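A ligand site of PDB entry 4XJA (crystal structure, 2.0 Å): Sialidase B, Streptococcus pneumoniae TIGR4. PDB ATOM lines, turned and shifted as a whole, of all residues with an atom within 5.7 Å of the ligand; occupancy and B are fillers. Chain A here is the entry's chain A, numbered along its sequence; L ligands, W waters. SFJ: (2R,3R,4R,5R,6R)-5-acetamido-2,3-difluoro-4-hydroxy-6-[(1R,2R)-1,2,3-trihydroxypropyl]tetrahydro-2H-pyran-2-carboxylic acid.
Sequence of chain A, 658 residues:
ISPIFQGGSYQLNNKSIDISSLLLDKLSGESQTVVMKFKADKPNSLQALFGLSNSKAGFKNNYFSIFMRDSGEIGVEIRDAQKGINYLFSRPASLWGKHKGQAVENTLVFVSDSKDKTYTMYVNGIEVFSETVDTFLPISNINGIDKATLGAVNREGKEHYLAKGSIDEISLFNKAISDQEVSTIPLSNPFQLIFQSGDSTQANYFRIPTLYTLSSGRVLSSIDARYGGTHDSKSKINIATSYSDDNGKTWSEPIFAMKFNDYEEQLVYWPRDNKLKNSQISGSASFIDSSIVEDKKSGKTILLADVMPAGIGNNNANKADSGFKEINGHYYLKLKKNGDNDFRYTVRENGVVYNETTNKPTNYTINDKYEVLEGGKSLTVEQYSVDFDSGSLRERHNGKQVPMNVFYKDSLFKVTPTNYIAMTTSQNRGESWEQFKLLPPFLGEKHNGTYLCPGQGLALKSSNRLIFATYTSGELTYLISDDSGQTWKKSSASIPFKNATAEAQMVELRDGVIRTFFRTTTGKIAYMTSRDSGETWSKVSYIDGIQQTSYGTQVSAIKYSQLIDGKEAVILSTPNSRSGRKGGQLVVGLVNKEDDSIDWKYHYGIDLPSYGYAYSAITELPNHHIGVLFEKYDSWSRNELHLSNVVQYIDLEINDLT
Merely in contact with the ligand: Ile 208 (3.5 Å), Ile 288 (3.7 Å), Asp 306 (3.5 Å), Tyr 451 (3.7 Å), Thr 501 (3.9 Å), Glu 503 (3.96 Å) and Trp 636 (3.8 Å).
Hydrophobic or aromatic side chains that line the ligand: Ile 208, Ile 288, Tyr 451, Tyr 615 and Trp 636.
Along chain A the residues within 4 Å of the ligand span positions 207 to 636.
The nearest printed residue that does not touch the ligand is Met 308 (4.3 Å).
O1B of the ligand is in salt-bridge range of NH1 of Arg 581, 2.9 Å away.
The side-chain carboxylate (OD1) of Asp 289 is in hydrogen-bond range of an oxygen (O4) of the ligand (2.6 Å).
O7 of the ligand sits at hydrogen-bond distance from OD2 of Asp 232 (2.5 Å).
An oxygen (O1A) of the ligand is in salt-bridge range of the guanidinium group (NH1) of Arg 519 (3.1 Å).
An oxygen (O4) of the ligand is in hydrogen-bond range of the guanidinium group (NH2) of Arg 226, 3.0 Å away.
The guanidinium group of Arg 207 lies within salt-bridge range of an oxygen (O1B) of the ligand (3.0 Å).
The side-chain amide nitrogen (ND2) of Asn 314 is in hydrogen-bond range of an oxygen (O9) of the ligand.
O1A of the ligand lies close to OH of Tyr 615 (3.2 Å).
The guanidinium group (NH2) of Arg 226 lies within salt-bridge range of the side-chain carboxylate (OD2) of Asp 224 (2.9 Å).
The guanidinium group (NH2) of Arg 207 is in hydrogen-bond range of the side-chain hydroxyl (OG) of Ser 635 (3.2 Å).
N of Asp 306 lies within hydrogen-bond range of O of Ile 288 (2.9 Å).
The guanidinium group of Arg 519 lies within hydrogen-bond range of the side-chain hydroxyl of Tyr 615.
The side-chain carboxylate (OD2) of Asp 232 lies within hydrogen-bond range of the side-chain amide nitrogen (ND2) of Asn 314, at 3.3 Å.
NH1 of Arg 581 lies within hydrogen-bond range of OG of Ser 635, 3.1 Å away.
The backbone carbonyl oxygen of Arg 207 is in hydrogen-bond range of the backbone NH of Asp 224, at 3.0 Å.
NE of Arg 519 sits close to O of Gly 552, at 3.3 Å.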
ATOM      1  N   ARG A 207       6.390   1.295 -30.247  1.00  0.00           N
ATOM      2  CA  ARG A 207       7.686   1.021 -29.659  1.00  0.00           C
ATOM      3  C   ARG A 207       8.402  -0.024 -30.499  1.00  0.00           C
ATOM      4  O   ARG A 207       7.781  -0.679 -31.339  1.00  0.00           O
ATOM      5  CB  ARG A 207       7.549   0.503 -28.228  1.00  0.00           C
ATOM      6  CG  ARG A 207       7.338   1.575 -27.128  1.00  0.00           C
ATOM      7  CD  ARG A 207       7.876   1.054 -25.770  1.00  0.00           C
ATOM      8  NE  ARG A 207       9.296   0.692 -25.869  1.00  0.00           N
ATOM      9  CZ  ARG A 207       9.986   0.060 -24.929  1.00  0.00           C
ATOM     10  NH1 ARG A 207       9.405  -0.307 -23.788  1.00  0.00           N
ATOM     11  NH2 ARG A 207      11.277  -0.215 -25.133  1.00  0.00           N
ATOM     12  N   ILE A 208       9.682  -0.203 -30.235  1.00  0.00           N
ATOM     13  CA  ILE A 208      10.475  -1.283 -30.838  1.00  0.00           C
ATOM     14  C   ILE A 208      10.618  -1.157 -32.363  1.00  0.00           C
ATOM     15  O   ILE A 208      10.208  -2.037 -33.108  1.00  0.00           O
ATOM     16  CB  ILE A 208       9.922  -2.688 -30.473  1.00  0.00           C
ATOM     17  CG1 ILE A 208       9.364  -2.719 -29.029  1.00  0.00           C
ATOM     18  CG2 ILE A 208      11.001  -3.734 -30.623  1.00  0.00           C
ATOM     19  CD1 ILE A 208      10.384  -2.427 -27.923  1.00  0.00           C
ATOM     20  N   ASP A 224       6.230  -2.359 -33.212  1.00  0.00           N
ATOM     21  CA  ASP A 224       5.093  -2.749 -32.390  1.00  0.00           C
ATOM     22  C   ASP A 224       4.065  -1.640 -32.486  1.00  0.00           C
ATOM     23  O   ASP A 224       4.336  -0.506 -32.055  1.00  0.00           O
ATOM     24  CB  ASP A 224       5.496  -2.800 -30.912  1.00  0.00           C
ATOM     25  CG  ASP A 224       6.217  -4.080 -30.524  1.00  0.00           C
ATOM     26  OD1 ASP A 224       6.860  -4.735 -31.380  1.00  0.00           O
ATOM     27  OD2 ASP A 224       6.148  -4.401 -29.322  1.00  0.00           O
ATOM     28  N   ARG A 226       1.259  -0.480 -30.577  1.00  0.00           N
ATOM     29  CA  ARG A 226       0.785  -0.787 -29.232  1.00  0.00           C
ATOM     30  C   ARG A 226      -0.483  -0.005 -28.907  1.00  0.00           C
ATOM     31  O   ARG A 226      -0.481   1.225 -28.890  1.00  0.00           O
ATOM     32  CB  ARG A 226       1.899  -0.521 -28.208  1.00  0.00           C
ATOM     33  CG  ARG A 226       3.153  -1.393 -28.429  1.00  0.00           C
ATOM     34  CD  ARG A 226       4.073  -1.421 -27.212  1.00  0.00           C
ATOM     35  NE  ARG A 226       5.137  -2.429 -27.360  1.00  0.00           N
ATOM     36  CZ  ARG A 226       6.049  -2.711 -26.430  1.00  0.00           C
ATOM     37  NH1 ARG A 226       6.048  -2.070 -25.267  1.00  0.00           N
ATOM     38  NH2 ARG A 226       6.965  -3.621 -26.671  1.00  0.00           N
ATOM     39  N   ASP A 232       4.355  -3.314 -22.502  1.00  0.00           N
ATOM     40  CA  ASP A 232       4.629  -4.590 -23.175  1.00  0.00           C
ATOM     41  C   ASP A 232       3.489  -5.544 -22.889  1.00  0.00           C
ATOM     42  O   ASP A 232       2.641  -5.261 -22.036  1.00  0.00           O
ATOM     43  CB  ASP A 232       5.964  -5.195 -22.708  1.00  0.00           C
ATOM     44  CG  ASP A 232       6.040  -5.339 -21.194  1.00  0.00           C
ATOM     45  OD1 ASP A 232       5.617  -4.413 -20.483  1.00  0.00           O
ATOM     46  OD2 ASP A 232       6.517  -6.393 -20.721  1.00  0.00           O
ATOM     47  N   SER A 233       3.458  -6.676 -23.592  1.00  0.00           N
ATOM     48  CA  SER A 233       2.455  -7.703 -23.341  1.00  0.00           C
ATOM     49  C   SER A 233       2.525  -8.081 -21.863  1.00  0.00           C
ATOM     50  O   SER A 233       3.619  -8.080 -21.296  1.00  0.00           O
ATOM     51  CB  SER A 233       2.736  -8.925 -24.211  1.00  0.00           C
ATOM     52  OG  SER A 233       2.812  -8.551 -25.581  1.00  0.00           O
ATOM     53  N   ILE A 288       4.906  -9.122 -30.235  1.00  0.00           N
ATOM     54  CA  ILE A 288       5.838  -8.164 -29.627  1.00  0.00           C
ATOM     55  C   ILE A 288       7.270  -8.473 -30.043  1.00  0.00           C
ATOM     56  O   ILE A 288       7.644  -9.644 -30.159  1.00  0.00           O
ATOM     57  CB  ILE A 288       5.668  -8.128 -28.071  1.00  0.00           C
ATOM     58  CG1 ILE A 288       6.638  -7.159 -27.413  1.00  0.00           C
ATOM     59  CG2 ILE A 288       5.787  -9.535 -27.459  1.00  0.00           C
ATOM     60  CD1 ILE A 288       6.318  -6.954 -25.946  1.00  0.00           C
ATOM     61  N   ASP A 289       8.062  -7.422 -30.291  1.00  0.00           N
ATOM     62  CA  ASP A 289       9.475  -7.529 -30.645  1.00  0.00           C
ATOM     63  C   ASP A 289       9.712  -8.201 -32.001  1.00  0.00           C
ATOM     64  O   ASP A 289       9.884  -9.417 -32.078  1.00  0.00           O
ATOM     65  CB  ASP A 289      10.278  -8.262 -29.562  1.00  0.00           C
ATOM     66  CG  ASP A 289      10.339  -7.491 -28.241  1.00  0.00           C
ATOM     67  OD1 ASP A 289       9.920  -6.321 -28.216  1.00  0.00           O
ATOM     68  OD2 ASP A 289      10.818  -8.066 -27.237  1.00  0.00           O
ATOM     69  N   ASP A 306       7.664 -12.227 -31.413  1.00  0.00           N
ATOM     70  CA  ASP A 306       7.101 -13.075 -30.362  1.00  0.00           C
ATOM     71  C   ASP A 306       5.586 -13.056 -30.475  1.00  0.00           C
ATOM     72  O   ASP A 306       4.997 -12.071 -30.911  1.00  0.00           O
ATOM     73  CB  ASP A 306       7.455 -12.557 -28.958  1.00  0.00           C
ATOM     74  CG  ASP A 306       8.960 -12.408 -28.725  1.00  0.00           C
ATOM     75  OD1 ASP A 306       9.796 -13.129 -29.335  1.00  0.00           O
ATOM     76  OD2 ASP A 306       9.312 -11.576 -27.862  1.00  0.00           O
ATOM     77  N   MET A 308       2.091 -13.778 -28.130  1.00  0.00           N
ATOM     78  CA  MET A 308       1.563 -13.988 -26.789  1.00  0.00           C
ATOM     79  C   MET A 308       0.076 -14.291 -26.902  1.00  0.00           C
ATOM     80  O   MET A 308      -0.660 -13.540 -27.543  1.00  0.00           O
ATOM     81  CB  MET A 308       1.740 -12.740 -25.950  1.00  0.00           C
ATOM     82  CG  MET A 308       3.178 -12.277 -25.816  1.00  0.00           C
ATOM     83  SD  MET A 308       4.098 -13.356 -24.726  1.00  0.00           S
ATOM     84  CE  MET A 308       5.670 -12.496 -24.789  1.00  0.00           C
ATOM     85  N   ASN A 314       5.607 -11.637 -20.917  1.00  0.00           N
ATOM     86  CA  ASN A 314       6.780 -12.311 -20.363  1.00  0.00           C
ATOM     87  C   ASN A 314       6.644 -12.553 -18.855  1.00  0.00           C
ATOM     88  O   ASN A 314       7.203 -13.516 -18.336  1.00  0.00           O
ATOM     89  CB  ASN A 314       8.081 -11.572 -20.693  1.00  0.00           C
ATOM     90  CG  ASN A 314       8.370 -10.424 -19.730  1.00  0.00           C
ATOM     91  OD1 ASN A 314       8.766 -10.641 -18.573  1.00  0.00           O
ATOM     92  ND2 ASN A 314       8.207  -9.190 -20.213  1.00  0.00           N
ATOM     93  N   TYR A 451      13.223 -15.475 -26.491  1.00  0.00           N
ATOM     94  CA  TYR A 451      12.709 -14.164 -26.837  1.00  0.00           C
ATOM     95  C   TYR A 451      13.475 -13.605 -28.008  1.00  0.00           C
ATOM     96  O   TYR A 451      14.703 -13.537 -27.979  1.00  0.00           O
ATOM     97  CB  TYR A 451      12.809 -13.250 -25.618  1.00  0.00           C
ATOM     98  CG  TYR A 451      11.800 -13.628 -24.555  1.00  0.00           C
ATOM     99  CD1 TYR A 451      10.455 -13.306 -24.720  1.00  0.00           C
ATOM    100  CD2 TYR A 451      12.190 -14.311 -23.407  1.00  0.00           C
ATOM    101  CE1 TYR A 451       9.523 -13.648 -23.765  1.00  0.00           C
ATOM    102  CE2 TYR A 451      11.250 -14.659 -22.443  1.00  0.00           C
ATOM    103  CZ  TYR A 451       9.929 -14.319 -22.627  1.00  0.00           C
ATOM    104  OH  TYR A 451       8.964 -14.647 -21.681  1.00  0.00           O
ATOM    105  N   TYR A 471      17.090 -14.634 -27.106  1.00  0.00           N
ATOM    106  CA  TYR A 471      17.691 -14.805 -25.777  1.00  0.00           C
ATOM    107  C   TYR A 471      16.780 -15.548 -24.807  1.00  0.00           C
ATOM    108  O   TYR A 471      15.548 -15.586 -24.975  1.00  0.00           O
ATOM    109  CB  TYR A 471      18.120 -13.452 -25.172  1.00  0.00           C
ATOM    110  CG  TYR A 471      16.971 -12.525 -24.879  1.00  0.00           C
ATOM    111  CD1 TYR A 471      16.471 -11.674 -25.865  1.00  0.00           C
ATOM    112  CD2 TYR A 471      16.395 -12.484 -23.611  1.00  0.00           C
ATOM    113  CE1 TYR A 471      15.412 -10.804 -25.596  1.00  0.00           C
ATOM    114  CE2 TYR A 471      15.327 -11.622 -23.322  1.00  0.00           C
ATOM    115  CZ  TYR A 471      14.853 -10.788 -24.320  1.00  0.00           C
ATOM    116  OH  TYR A 471      13.791  -9.933 -24.051  1.00  0.00           O
ATOM    117  N   THR A 501      17.798  -9.397 -20.046  1.00  0.00           N
ATOM    118  CA  THR A 501      17.103  -9.078 -21.286  1.00  0.00           C
ATOM    119  C   THR A 501      18.206  -8.891 -22.331  1.00  0.00           C
ATOM    120  O   THR A 501      18.578  -7.771 -22.673  1.00  0.00           O
ATOM    121  CB  THR A 501      16.242  -7.821 -21.123  1.00  0.00           C
ATOM    122  OG1 THR A 501      15.378  -8.006 -19.989  1.00  0.00           O
ATOM    123  CG2 THR A 501      15.388  -7.552 -22.345  1.00  0.00           C
ATOM    124  N   GLU A 503      19.135  -8.586 -25.342  1.00  0.00           N
ATOM    125  CA  GLU A 503      18.816  -8.205 -26.719  1.00  0.00           C
ATOM    126  C   GLU A 503      20.117  -8.021 -27.495  1.00  0.00           C
ATOM    127  O   GLU A 503      20.985  -7.240 -27.088  1.00  0.00           O
ATOM    128  CB  GLU A 503      17.938  -6.947 -26.746  1.00  0.00           C
ATOM    129  CG  GLU A 503      16.529  -7.159 -26.123  1.00  0.00           C
ATOM    130  CD  GLU A 503      15.865  -5.870 -25.678  1.00  0.00           C
ATOM    131  OE1 GLU A 503      14.611  -5.819 -25.579  1.00  0.00           O
ATOM    132  OE2 GLU A 503      16.602  -4.890 -25.419  1.00  0.00           O
ATOM    133  N   ARG A 519      22.827  -6.382 -24.998  1.00  0.00           N
ATOM    134  CA  ARG A 519      22.441  -5.771 -23.726  1.00  0.00           C
ATOM    135  C   ARG A 519      22.705  -6.747 -22.586  1.00  0.00           C
ATOM    136  O   ARG A 519      22.503  -7.962 -22.732  1.00  0.00           O
ATOM    137  CB  ARG A 519      20.941  -5.442 -23.779  1.00  0.00           C
ATOM    138  CG  ARG A 519      20.298  -4.899 -22.510  1.00  0.00           C
ATOM    139  CD  ARG A 519      18.810  -4.718 -22.762  1.00  0.00           C
ATOM    140  NE  ARG A 519      18.030  -4.449 -21.550  1.00  0.00           N
ATOM    141  CZ  ARG A 519      16.743  -4.133 -21.565  1.00  0.00           C
ATOM    142  NH1 ARG A 519      16.094  -4.042 -22.728  1.00  0.00           N
ATOM    143  NH2 ARG A 519      16.102  -3.920 -20.426  1.00  0.00           N
ATOM    144  N   GLY A 552      19.768  -1.826 -18.697  1.00  0.00           N
ATOM    145  CA  GLY A 552      20.241  -1.835 -20.072  1.00  0.00           C
ATOM    146  C   GLY A 552      19.172  -1.460 -21.086  1.00  0.00           C
ATOM    147  O   GLY A 552      18.002  -1.281 -20.749  1.00  0.00           O
ATOM    148  N   ARG A 581      17.411   6.124 -19.941  1.00  0.00           N
ATOM    149  CA  ARG A 581      17.498   5.938 -21.386  1.00  0.00           C
ATOM    150  C   ARG A 581      17.495   7.318 -22.020  1.00  0.00           C
ATOM    151  O   ARG A 581      16.453   7.863 -22.392  1.00  0.00           O
ATOM    152  CB  ARG A 581      16.363   5.040 -21.898  1.00  0.00           C
ATOM    153  CG  ARG A 581      16.466   3.589 -21.329  1.00  0.00           C
ATOM    154  CD  ARG A 581      15.365   2.676 -21.812  1.00  0.00           C
ATOM    155  NE  ARG A 581      15.700   1.261 -21.602  1.00  0.00           N
ATOM    156  CZ  ARG A 581      14.853   0.259 -21.741  1.00  0.00           C
ATOM    157  NH1 ARG A 581      13.597   0.497 -22.102  1.00  0.00           N
ATOM    158  NH2 ARG A 581      15.254  -0.988 -21.531  1.00  0.00           N
ATOM    159  N   TYR A 615      15.107   2.449 -27.376  1.00  0.00           N
ATOM    160  CA  TYR A 615      15.311   1.454 -28.422  1.00  0.00           C
ATOM    161  C   TYR A 615      15.506   2.163 -29.751  1.00  0.00           C
ATOM    162  O   TYR A 615      14.935   3.233 -29.981  1.00  0.00           O
ATOM    163  CB  TYR A 615      14.123   0.504 -28.526  1.00  0.00           C
ATOM    164  CG  TYR A 615      14.106  -0.622 -27.505  1.00  0.00           C
ATOM    165  CD1 TYR A 615      14.342  -0.390 -26.149  1.00  0.00           C
ATOM    166  CD2 TYR A 615      13.790  -1.923 -27.896  1.00  0.00           C
ATOM    167  CE1 TYR A 615      14.287  -1.439 -25.212  1.00  0.00           C
ATOM    168  CE2 TYR A 615      13.730  -2.963 -26.979  1.00  0.00           C
ATOM    169  CZ  TYR A 615      13.974  -2.723 -25.642  1.00  0.00           C
ATOM    170  OH  TYR A 615      13.911  -3.776 -24.746  1.00  0.00           O
ATOM    171  N   SER A 635      11.887   5.055 -22.369  1.00  0.00           N
ATOM    172  CA  SER A 635      10.861   4.004 -22.361  1.00  0.00           C
ATOM    173  C   SER A 635      10.944   3.092 -21.136  1.00  0.00           C
ATOM    174  O   SER A 635      10.167   2.132 -21.013  1.00  0.00           O
ATOM    175  CB  SER A 635      10.901   3.191 -23.654  1.00  0.00           C
ATOM    176  OG  SER A 635      12.156   2.561 -23.830  1.00  0.00           O
ATOM    177  N   TRP A 636      11.866   3.377 -20.220  1.00  0.00           N
ATOM    178  CA  TRP A 636      11.907   2.663 -18.932  1.00  0.00           C
ATOM    179  C   TRP A 636      11.168   3.445 -17.858  1.00  0.00           C
ATOM    180  O   TRP A 636      10.470   2.859 -17.030  1.00  0.00           O
ATOM    181  CB  TRP A 636      13.349   2.449 -18.471  1.00  0.00           C
ATOM    182  CG  TRP A 636      13.471   1.518 -17.288  1.00  0.00           C
ATOM    183  CD1 TRP A 636      13.569   1.864 -15.964  1.00  0.00           C
ATOM    184  CD2 TRP A 636      13.519   0.093 -17.337  1.00  0.00           C
ATOM    185  NE1 TRP A 636      13.685   0.736 -15.184  1.00  0.00           N
ATOM    186  CE2 TRP A 636      13.650  -0.367 -15.994  1.00  0.00           C
ATOM    187  CE3 TRP A 636      13.459  -0.855 -18.369  1.00  0.00           C
ATOM    188  CZ2 TRP A 636      13.732  -1.720 -15.679  1.00  0.00           C
ATOM    189  CZ3 TRP A 636      13.541  -2.208 -18.043  1.00  0.00           C
ATOM    190  CH2 TRP A 636      13.666  -2.624 -16.707  1.00  0.00           C
HETATM  191  C11 SFJ L   1       9.041  -9.855 -24.847  1.00  0.00           C
HETATM  192  C9  SFJ L   1      11.527  -7.521 -19.561  1.00  0.00           C
HETATM  193  C10 SFJ L   1       9.119  -8.549 -24.064  1.00  0.00           C
HETATM  194  C1  SFJ L   1      12.329  -2.886 -22.329  1.00  0.00           C
HETATM  195  C7  SFJ L   1      10.299  -6.571 -21.370  1.00  0.00           C
HETATM  196  C4  SFJ L   1      10.411  -5.175 -24.930  1.00  0.00           C
HETATM  197  C3  SFJ L   1      10.616  -3.804 -24.183  1.00  0.00           C
HETATM  198  C5  SFJ L   1      10.067  -6.284 -23.906  1.00  0.00           C
HETATM  199  C6  SFJ L   1      11.053  -6.335 -22.751  1.00  0.00           C
HETATM  200  C2  SFJ L   1      11.331  -4.027 -22.697  1.00  0.00           C
HETATM  201  N5  SFJ L   1       9.953  -7.600 -24.529  1.00  0.00           N
HETATM  202  O10 SFJ L   1       8.401  -8.391 -23.099  1.00  0.00           O
HETATM  203  O9  SFJ L   1      10.426  -8.333 -19.347  1.00  0.00           O
HETATM  204  O1A SFJ L   1      13.348  -3.184 -21.701  1.00  0.00           O
HETATM  205  O8  SFJ L   1      12.105  -5.366 -20.129  1.00  0.00           O
HETATM  206  O7  SFJ L   1       8.962  -6.067 -21.242  1.00  0.00           O
HETATM  207  O4  SFJ L   1       9.511  -5.133 -25.955  1.00  0.00           O
HETATM  208  O6  SFJ L   1      11.940  -5.262 -22.707  1.00  0.00           O
HETATM  209  FAI SFJ L   1       9.659  -3.338 -24.100  1.00  0.00           F
HETATM  210  FAJ SFJ L   1      10.601  -3.942 -21.687  1.00  0.00           F
HETATM  211  O1B SFJ L   1      11.918  -1.762 -22.637  1.00  0.00           O
HETATM  212  C8  SFJ L   1      11.021  -6.232 -20.029  1.00  0.00           C
HETATM  213  O   HOH W   1       5.819  -9.129 -22.373  1.00  0.00           O
